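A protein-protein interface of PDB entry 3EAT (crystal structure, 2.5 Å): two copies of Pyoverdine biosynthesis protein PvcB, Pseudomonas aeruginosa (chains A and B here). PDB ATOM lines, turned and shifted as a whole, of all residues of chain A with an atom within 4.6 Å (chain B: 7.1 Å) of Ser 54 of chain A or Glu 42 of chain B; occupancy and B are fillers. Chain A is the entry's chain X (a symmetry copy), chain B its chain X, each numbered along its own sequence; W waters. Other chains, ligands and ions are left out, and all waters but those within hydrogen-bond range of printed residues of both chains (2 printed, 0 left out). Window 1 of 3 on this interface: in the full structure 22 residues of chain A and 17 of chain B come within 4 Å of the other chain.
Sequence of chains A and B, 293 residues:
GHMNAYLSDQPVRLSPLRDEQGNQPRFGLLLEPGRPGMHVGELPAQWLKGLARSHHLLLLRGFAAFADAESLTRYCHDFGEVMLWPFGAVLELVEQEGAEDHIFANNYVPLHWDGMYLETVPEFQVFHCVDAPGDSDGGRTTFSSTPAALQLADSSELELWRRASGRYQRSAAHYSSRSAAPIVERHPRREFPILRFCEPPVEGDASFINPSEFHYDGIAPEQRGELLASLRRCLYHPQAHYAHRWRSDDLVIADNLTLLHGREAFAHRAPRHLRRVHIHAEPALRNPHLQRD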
ATOM      1  N   GLY A  50      -9.907  24.294  -2.775  1.00  0.00           N
ATOM      2  CA  GLY A  50     -10.505  23.404  -1.773  1.00  0.00           C
ATOM      3  C   GLY A  50     -11.993  23.169  -2.005  1.00  0.00           C
ATOM      4  O   GLY A  50     -12.447  22.018  -2.032  1.00  0.00           O
ATOM      5  N   LEU A  51     -12.751  24.252  -2.201  1.00  0.00           N
ATOM      6  CA  LEU A  51     -14.178  24.136  -2.521  1.00  0.00           C
ATOM      7  C   LEU A  51     -14.412  23.397  -3.834  1.00  0.00           C
ATOM      8  O   LEU A  51     -15.336  22.590  -3.946  1.00  0.00           O
ATOM      9  CB  LEU A  51     -14.820  25.518  -2.599  1.00  0.00           C
ATOM     10  CG  LEU A  51     -14.773  26.346  -1.318  1.00  0.00           C
ATOM     11  CD1 LEU A  51     -15.398  27.686  -1.609  1.00  0.00           C
ATOM     12  CD2 LEU A  51     -15.517  25.615  -0.218  1.00  0.00           C
ATOM     13  N   ALA A  52     -13.571  23.672  -4.828  1.00  0.00           N
ATOM     14  CA  ALA A  52     -13.734  23.033  -6.125  1.00  0.00           C
ATOM     15  C   ALA A  52     -13.516  21.527  -6.011  1.00  0.00           C
ATOM     16  O   ALA A  52     -14.154  20.737  -6.713  1.00  0.00           O
ATOM     17  CB  ALA A  52     -12.805  23.648  -7.156  1.00  0.00           C
ATOM     18  N   ARG A  53     -12.639  21.133  -5.096  1.00  0.00           N
ATOM     19  CA  ARG A  53     -12.357  19.722  -4.891  1.00  0.00           C
ATOM     20  C   ARG A  53     -13.462  18.942  -4.179  1.00  0.00           C
ATOM     21  O   ARG A  53     -13.589  17.731  -4.379  1.00  0.00           O
ATOM     22  CB  ARG A  53     -11.044  19.563  -4.149  1.00  0.00           C
ATOM     23  CG  ARG A  53      -9.900  19.622  -5.071  1.00  0.00           C
ATOM     24  CD  ARG A  53      -8.602  19.653  -4.328  1.00  0.00           C
ATOM     25  NE  ARG A  53      -7.513  19.817  -5.275  1.00  0.00           N
ATOM     26  CZ  ARG A  53      -6.424  20.543  -5.039  1.00  0.00           C
ATOM     27  NH1 ARG A  53      -6.301  21.191  -3.891  1.00  0.00           N
ATOM     28  NH2 ARG A  53      -5.479  20.643  -5.973  1.00  0.00           N
ATOM     29  N   SER A  54     -14.246  19.619  -3.345  1.00  0.00           N
ATOM     30  CA  SER A  54     -15.285  18.920  -2.579  1.00  0.00           C
ATOM     31  C   SER A  54     -16.693  19.158  -3.138  1.00  0.00           C
ATOM     32  O   SER A  54     -17.570  18.296  -2.999  1.00  0.00           O
ATOM     33  CB  SER A  54     -15.231  19.331  -1.112  1.00  0.00           C
ATOM     34  OG  SER A  54     -15.412  20.734  -1.001  1.00  0.00           O
ATOM     35  N   HIS A  55     -16.905  20.322  -3.752  1.00  0.00           N
ATOM     36  CA  HIS A  55     -18.172  20.618  -4.408  1.00  0.00           C
ATOM     37  C   HIS A  55     -18.112  20.337  -5.914  1.00  0.00           C
ATOM     38  O   HIS A  55     -19.147  20.344  -6.597  1.00  0.00           O
ATOM     39  CB  HIS A  55     -18.546  22.081  -4.201  1.00  0.00           C
ATOM     40  CG  HIS A  55     -18.786  22.459  -2.773  1.00  0.00           C
ATOM     41  ND1 HIS A  55     -19.979  22.207  -2.124  1.00  0.00           N
ATOM     42  CD2 HIS A  55     -17.992  23.095  -1.878  1.00  0.00           C
ATOM     43  CE1 HIS A  55     -19.902  22.667  -0.887  1.00  0.00           C
ATOM     44  NE2 HIS A  55     -18.706  23.208  -0.713  1.00  0.00           N
ATOM     45  N   HIS A  56     -16.893  20.145  -6.430  1.00  0.00           N
ATOM     46  CA  HIS A  56     -16.650  19.745  -7.827  1.00  0.00           C
ATOM     47  C   HIS A  56     -16.980  20.774  -8.885  1.00  0.00           C
ATOM     48  O   HIS A  56     -16.392  20.732  -9.957  1.00  0.00           O
ATOM     49  CB  HIS A  56     -17.324  18.419  -8.169  1.00  0.00           C
ATOM     50  CG  HIS A  56     -17.062  17.351  -7.165  1.00  0.00           C
ATOM     51  ND1 HIS A  56     -15.788  17.005  -6.767  1.00  0.00           N
ATOM     52  CD2 HIS A  56     -17.904  16.550  -6.468  1.00  0.00           C
ATOM     53  CE1 HIS A  56     -15.854  16.041  -5.868  1.00  0.00           C
ATOM     54  NE2 HIS A  56     -17.128  15.746  -5.666  1.00  0.00           N
ATOM     55  N   ARG A 190      -7.119  11.166  -4.759  1.00  0.00           N
ATOM     56  CA  ARG A 190      -7.843  11.186  -3.483  1.00  0.00           C
ATOM     57  C   ARG A 190      -8.689   9.926  -3.239  1.00  0.00           C
ATOM     58  O   ARG A 190      -9.497   9.877  -2.302  1.00  0.00           O
ATOM     59  CB  ARG A 190      -8.724  12.448  -3.396  1.00  0.00           C
ATOM     60  CG  ARG A 190      -7.961  13.756  -3.558  1.00  0.00           C
ATOM     61  CD  ARG A 190      -8.852  14.932  -3.319  1.00  0.00           C
ATOM     62  NE  ARG A 190      -9.546  15.367  -4.519  1.00  0.00           N
ATOM     63  CZ  ARG A 190     -10.801  15.804  -4.530  1.00  0.00           C
ATOM     64  NH1 ARG A 190     -11.504  15.815  -3.399  1.00  0.00           N
ATOM     65  NH2 ARG A 190     -11.360  16.216  -5.672  1.00  0.00           N
ATOM     66  N   PHE A 192     -11.328   8.286  -3.889  1.00  0.00           N
ATOM     67  CA  PHE A 192     -12.758   7.990  -3.864  1.00  0.00           C
ATOM     68  C   PHE A 192     -13.238   7.443  -5.220  1.00  0.00           C
ATOM     69  O   PHE A 192     -12.595   7.688  -6.240  1.00  0.00           O
ATOM     70  CB  PHE A 192     -13.585   9.178  -3.345  1.00  0.00           C
ATOM     71  CG  PHE A 192     -13.454  10.434  -4.154  1.00  0.00           C
ATOM     72  CD1 PHE A 192     -14.361  10.720  -5.168  1.00  0.00           C
ATOM     73  CD2 PHE A 192     -12.459  11.354  -3.873  1.00  0.00           C
ATOM     74  CE1 PHE A 192     -14.252  11.901  -5.924  1.00  0.00           C
ATOM     75  CE2 PHE A 192     -12.351  12.541  -4.616  1.00  0.00           C
ATOM     76  CZ  PHE A 192     -13.245  12.808  -5.637  1.00  0.00           C
ATOM     77  N   ASP B   9     -18.160  25.850   5.030  1.00  0.00           N
ATOM     78  CA  ASP B   9     -18.392  26.083   3.621  1.00  0.00           C
ATOM     79  C   ASP B   9     -18.093  24.793   2.825  1.00  0.00           C
ATOM     80  O   ASP B   9     -18.367  24.722   1.625  1.00  0.00           O
ATOM     81  CB  ASP B   9     -17.633  27.321   3.108  1.00  0.00           C
ATOM     82  CG  ASP B   9     -16.189  27.448   3.663  1.00  0.00           C
ATOM     83  OD1 ASP B   9     -15.637  26.499   4.311  1.00  0.00           O
ATOM     84  OD2 ASP B   9     -15.597  28.543   3.442  1.00  0.00           O
ATOM     85  N   GLN B  10     -17.561  23.777   3.514  1.00  0.00           N
ATOM     86  CA  GLN B  10     -17.396  22.430   2.970  1.00  0.00           C
ATOM     87  C   GLN B  10     -18.687  21.595   3.089  1.00  0.00           C
ATOM     88  O   GLN B  10     -19.530  21.860   3.959  1.00  0.00           O
ATOM     89  CB  GLN B  10     -16.271  21.706   3.706  1.00  0.00           C
ATOM     90  CG  GLN B  10     -14.902  22.361   3.618  1.00  0.00           C
ATOM     91  CD  GLN B  10     -14.312  22.376   2.210  1.00  0.00           C
ATOM     92  OE1 GLN B  10     -13.584  23.308   1.852  1.00  0.00           O
ATOM     93  NE2 GLN B  10     -14.600  21.347   1.425  1.00  0.00           N
ATOM     94  N   PRO B  11     -18.845  20.568   2.229  1.00  0.00           N
ATOM     95  CA  PRO B  11     -20.059  19.719   2.275  1.00  0.00           C
ATOM     96  C   PRO B  11     -19.993  18.687   3.416  1.00  0.00           C
ATOM     97  O   PRO B  11     -19.932  17.477   3.179  1.00  0.00           O
ATOM     98  CB  PRO B  11     -20.051  19.039   0.909  1.00  0.00           C
ATOM     99  CG  PRO B  11     -18.555  18.896   0.573  1.00  0.00           C
ATOM    100  CD  PRO B  11     -17.894  20.131   1.184  1.00  0.00           C
ATOM    101  N   ARG B  35     -23.219  14.500   2.111  1.00  0.00           N
ATOM    102  CA  ARG B  35     -23.905  13.891   0.969  1.00  0.00           C
ATOM    103  C   ARG B  35     -23.963  12.377   1.172  1.00  0.00           C
ATOM    104  O   ARG B  35     -23.006  11.790   1.679  1.00  0.00           O
ATOM    105  CB  ARG B  35     -23.163  14.167  -0.346  1.00  0.00           C
ATOM    106  CG  ARG B  35     -23.144  15.613  -0.831  1.00  0.00           C
ATOM    107  CD  ARG B  35     -22.580  15.685  -2.258  1.00  0.00           C
ATOM    108  NE  ARG B  35     -21.152  15.358  -2.301  1.00  0.00           N
ATOM    109  CZ  ARG B  35     -20.184  16.258  -2.440  1.00  0.00           C
ATOM    110  NH1 ARG B  35     -20.484  17.551  -2.563  1.00  0.00           N
ATOM    111  NH2 ARG B  35     -18.915  15.867  -2.443  1.00  0.00           N
ATOM    112  N   PRO B  36     -25.066  11.732   0.745  1.00  0.00           N
ATOM    113  CA  PRO B  36     -25.114  10.265   0.801  1.00  0.00           C
ATOM    114  C   PRO B  36     -23.903   9.608   0.125  1.00  0.00           C
ATOM    115  O   PRO B  36     -23.527   9.988  -0.984  1.00  0.00           O
ATOM    116  CB  PRO B  36     -26.395   9.934   0.026  1.00  0.00           C
ATOM    117  CG  PRO B  36     -27.263  11.126   0.232  1.00  0.00           C
ATOM    118  CD  PRO B  36     -26.309  12.304   0.197  1.00  0.00           C
ATOM    119  N   GLY B  37     -23.300   8.638   0.797  1.00  0.00           N
ATOM    120  CA  GLY B  37     -22.178   7.883   0.231  1.00  0.00           C
ATOM    121  C   GLY B  37     -20.829   8.603   0.158  1.00  0.00           C
ATOM    122  O   GLY B  37     -19.883   8.073  -0.417  1.00  0.00           O
ATOM    123  N   MET B  38     -20.714   9.788   0.756  1.00  0.00           N
ATOM    124  CA  MET B  38     -19.469  10.554   0.696  1.00  0.00           C
ATOM    125  C   MET B  38     -18.285   9.757   1.235  1.00  0.00           C
ATOM    126  O   MET B  38     -18.410   9.032   2.233  1.00  0.00           O
ATOM    127  CB  MET B  38     -19.620  11.862   1.448  1.00  0.00           C
ATOM    128  CG  MET B  38     -18.439  12.782   1.345  1.00  0.00           C
ATOM    129  SD  MET B  38     -18.772  14.384   2.094  1.00  0.00           S
ATOM    130  CE  MET B  38     -19.745  15.164   0.823  1.00  0.00           C
ATOM    131  N   HIS B  39     -17.149   9.880   0.545  1.00  0.00           N
ATOM    132  CA  HIS B  39     -15.888   9.229   0.900  1.00  0.00           C
ATOM    133  C   HIS B  39     -14.990  10.286   1.544  1.00  0.00           C
ATOM    134  O   HIS B  39     -15.136  11.462   1.249  1.00  0.00           O
ATOM    135  CB  HIS B  39     -15.262   8.703  -0.390  1.00  0.00           C
ATOM    136  CG  HIS B  39     -14.070   7.826  -0.195  1.00  0.00           C
ATOM    137  ND1 HIS B  39     -12.814   8.327   0.090  1.00  0.00           N
ATOM    138  CD2 HIS B  39     -13.929   6.479  -0.289  1.00  0.00           C
ATOM    139  CE1 HIS B  39     -11.957   7.321   0.191  1.00  0.00           C
ATOM    140  NE2 HIS B  39     -12.607   6.191  -0.043  1.00  0.00           N
ATOM    141  N   VAL B  40     -14.062   9.897   2.417  1.00  0.00           N
ATOM    142  CA  VAL B  40     -13.231  10.904   3.090  1.00  0.00           C
ATOM    143  C   VAL B  40     -12.399  11.689   2.094  1.00  0.00           C
ATOM    144  O   VAL B  40     -12.058  12.851   2.343  1.00  0.00           O
ATOM    145  CB  VAL B  40     -12.290  10.331   4.198  1.00  0.00           C
ATOM    146  CG1 VAL B  40     -13.051   9.500   5.221  1.00  0.00           C
ATOM    147  CG2 VAL B  40     -11.205   9.511   3.600  1.00  0.00           C
ATOM    148  N   GLY B  41     -12.089  11.058   0.962  1.00  0.00           N
ATOM    149  CA  GLY B  41     -11.195  11.642  -0.040  1.00  0.00           C
ATOM    150  C   GLY B  41     -11.788  12.857  -0.720  1.00  0.00           C
ATOM    151  O   GLY B  41     -11.056  13.689  -1.272  1.00  0.00           O
ATOM    152  N   GLU B  42     -13.112  12.979  -0.653  1.00  0.00           N
ATOM    153  CA  GLU B  42     -13.818  14.129  -1.248  1.00  0.00           C
ATOM    154  C   GLU B  42     -13.558  15.455  -0.545  1.00  0.00           C
ATOM    155  O   GLU B  42     -13.827  16.513  -1.104  1.00  0.00           O
ATOM    156  CB  GLU B  42     -15.316  13.851  -1.368  1.00  0.00           C
ATOM    157  CG  GLU B  42     -15.586  12.600  -2.215  1.00  0.00           C
ATOM    158  CD  GLU B  42     -17.045  12.241  -2.309  1.00  0.00           C
ATOM    159  OE1 GLU B  42     -17.852  13.092  -2.741  1.00  0.00           O
ATOM    160  OE2 GLU B  42     -17.382  11.083  -1.986  1.00  0.00           O
ATOM    161  N   LEU B  43     -13.025  15.408   0.670  1.00  0.00           N
ATOM    162  CA  LEU B  43     -12.732  16.635   1.394  1.00  0.00           C
ATOM    163  C   LEU B  43     -11.288  16.993   1.095  1.00  0.00           C
ATOM    164  O   LEU B  43     -10.460  16.093   0.930  1.00  0.00           O
ATOM    165  CB  LEU B  43     -12.971  16.448   2.901  1.00  0.00           C
ATOM    166  CG  LEU B  43     -14.417  16.088   3.290  1.00  0.00           C
ATOM    167  CD1 LEU B  43     -14.554  15.721   4.749  1.00  0.00           C
ATOM    168  CD2 LEU B  43     -15.341  17.236   2.946  1.00  0.00           C
ATOM    169  N   PRO B  44     -10.981  18.301   1.006  1.00  0.00           N
ATOM    170  CA  PRO B  44      -9.613  18.695   0.672  1.00  0.00           C
ATOM    171  C   PRO B  44      -8.697  18.524   1.875  1.00  0.00           C
ATOM    172  O   PRO B  44      -8.926  19.137   2.917  1.00  0.00           O
ATOM    173  CB  PRO B  44      -9.737  20.192   0.305  1.00  0.00           C
ATOM    174  CG  PRO B  44     -11.190  20.585   0.556  1.00  0.00           C
ATOM    175  CD  PRO B  44     -11.861  19.461   1.252  1.00  0.00           C
ATOM    176  N   ALA B  45      -7.667  17.701   1.711  1.00  0.00           N
ATOM    177  CA  ALA B  45      -6.633  17.458   2.726  1.00  0.00           C
ATOM    178  C   ALA B  45      -6.049  18.720   3.345  1.00  0.00           C
ATOM    179  O   ALA B  45      -5.829  18.766   4.566  1.00  0.00           O
ATOM    180  CB  ALA B  45      -5.504  16.605   2.130  1.00  0.00           C
ATOM    181  N   PHE B  63     -18.209   8.141   6.980  1.00  0.00           N
ATOM    182  CA  PHE B  63     -17.738   8.244   5.582  1.00  0.00           C
ATOM    183  C   PHE B  63     -17.476   6.861   5.006  1.00  0.00           C
ATOM    184  O   PHE B  63     -17.165   5.936   5.738  1.00  0.00           O
ATOM    185  CB  PHE B  63     -16.448   9.081   5.496  1.00  0.00           C
ATOM    186  CG  PHE B  63     -16.652  10.545   5.759  1.00  0.00           C
ATOM    187  CD1 PHE B  63     -16.829  11.429   4.710  1.00  0.00           C
ATOM    188  CD2 PHE B  63     -16.690  11.037   7.067  1.00  0.00           C
ATOM    189  CE1 PHE B  63     -17.043  12.797   4.946  1.00  0.00           C
ATOM    190  CE2 PHE B  63     -16.892  12.403   7.314  1.00  0.00           C
ATOM    191  CZ  PHE B  63     -17.075  13.282   6.248  1.00  0.00           C
ATOM    192  N   ALA B  64     -17.580   6.724   3.693  1.00  0.00           N
ATOM    193  CA  ALA B  64     -17.161   5.490   3.035  1.00  0.00           C
ATOM    194  C   ALA B  64     -15.675   5.196   3.233  1.00  0.00           C
ATOM    195  O   ALA B  64     -14.829   6.104   3.348  1.00  0.00           O
ATOM    196  CB  ALA B  64     -17.516   5.492   1.554  1.00  0.00           C
ATOM    197  N   TYR B  75      -3.846   7.703  -0.527  1.00  0.00           N
ATOM    198  CA  TYR B  75      -4.509   8.864   0.035  1.00  0.00           C
ATOM    199  C   TYR B  75      -3.536   9.682   0.873  1.00  0.00           C
ATOM    200  O   TYR B  75      -3.431  10.892   0.695  1.00  0.00           O
ATOM    201  CB  TYR B  75      -5.744   8.475   0.878  1.00  0.00           C
ATOM    202  CG  TYR B  75      -6.315   9.662   1.627  1.00  0.00           C
ATOM    203  CD1 TYR B  75      -7.191  10.545   0.994  1.00  0.00           C
ATOM    204  CD2 TYR B  75      -5.942   9.935   2.945  1.00  0.00           C
ATOM    205  CE1 TYR B  75      -7.699  11.645   1.659  1.00  0.00           C
ATOM    206  CE2 TYR B  75      -6.440  11.050   3.616  1.00  0.00           C
ATOM    207  CZ  TYR B  75      -7.327  11.895   2.964  1.00  0.00           C
ATOM    208  OH  TYR B  75      -7.844  13.015   3.604  1.00  0.00           O
HETATM  209  O   HOH W   1     -19.141  13.866  -5.040  1.00  0.00           O
HETATM  210  O   HOH W   2     -11.451  25.426   0.705  1.00  0.00           O
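Water W1 lies within hydrogen-bond range of the side-chain carboxylate (OE1) of Glu 42 of chain B (2.7 Å), a ring nitrogen (NE2) of His 56 of chain A (2.8 Å) and the guanidinium group (NH2) of Arg 35 of chain B (3.3 Å). Water W2 lies within hydrogen-bond range of the side-chain amide oxygen of Gln 10 of chain B (3.2 Å) and the backbone NH of Leu 51 of chain A (3.4 Å).
Among the printed residues, merely in contact across the chains: Gly 50 of chain A with Pro 44 of chain B, Leu 51 of chain A with Asp 9 of chain B, Leu 51 of chain A with Gln 10 of chain B, Arg 53 of chain A with Glu 42 of chain B, Ser 54 of chain A with Pro 11 of chain B, Ser 54 of chain A with Glu 42 of chain B, His 55 of chain A with Gln 10 of chain B, His 55 of chain A with Pro 11 of chain B, His 56 of chain A with Arg 35 of chain B, Phe 192 of chain A with His 39 of chain B, Phe 192 of chain A with Gly 41 of chain B and Phe 192 of chain A with Glu 42 of chain B.
The side-chain amide nitrogen of Gln 10 of chain B is in hydrogen-bond range of the side-chain hydroxyl of Ser 54 of chain A. The guanidinium group of Arg 190 of chain A lies within hydrogen-bond range of the backbone carbonyl oxygen of Gly 41 of chain B. A ring nitrogen (NE2) of His 55 of chain A is in hydrogen-bond range of the backbone carbonyl oxygen (O) of Asp 9 of chain B, at 2.8 Å. The guanidinium group of Arg 190 of chain A sits at hydrogen-bond distance from the backbone carbonyl oxygen of Glu 42 of chain B, at 3.3 Å. The guanidinium group of Arg 35 of chain B sits at hydrogen-bond distance from the backbone carbonyl oxygen of Ser 54 of chain A, at 2.8 Å.
Printed residues of chain B that touch a printed residue of chain A: Asp 9, Gln 10, Pro 11, Arg 35, His 39, Gly 41, Glu 42 and Pro 44. Along chain B the printed residues that touch a printed residue of chain A span positions 9 to 44. Of the 9 printed residues of chain A, 8 touch a printed residue of chain B. Hydrophobic or aromatic side chains of chain A within 4 Å of the printed part of chain B: Leu 51, His 55, His 56 and Phe 192.
The backbone carbonyl oxygen (O) of Arg 53 of chain A lies within hydrogen-bond range of the guanidinium group (NH2) of Arg 190 of chain A. The backbone carbonyl oxygen (O) of Leu 51 of chain A is in hydrogen-bond range of the side-chain hydroxyl (OG) of Ser 54 of chain A, at 3.5 Å. OE1 of Glu 42 of chain B is in salt-bridge range of NH2 of Arg 35 of chain B, at 3.0 Å. The backbone NH (N) of Gly 41 of chain B sits at hydrogen-bond distance from a ring nitrogen (ND1) of His 39 of chain B, at 3.0 Å. ND1 of His 56 of chain A sits close to O of Arg 53 of chain A (3.3 Å). The side-chain hydroxyl of Ser 54 of chain A is in hydrogen-bond range of the backbone carbonyl oxygen of Gly 50 of chain A.
Ser 54 of chain A touches four residues of chain B. Of the printed residues of chain B, Arg 190 of chain A touches Gly 41 (3.0 Å) and Glu 42 (3.3 Å). Of the printed residues of chain B, Gly 50 of chain A touches Pro 44 (3.2 Å). Of the printed residues of chain B, His 56 of chain A touches Arg 35 (3.7 Å). The nearest residue of chain B that does not touch Ser 54 of chain A is Pro 44 of chain B (4.1 Å). The nearest printed residue of chain A that does not touch His 39 of chain B is Arg 190 of chain A (4.3 Å).
No position is printed for both chains.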
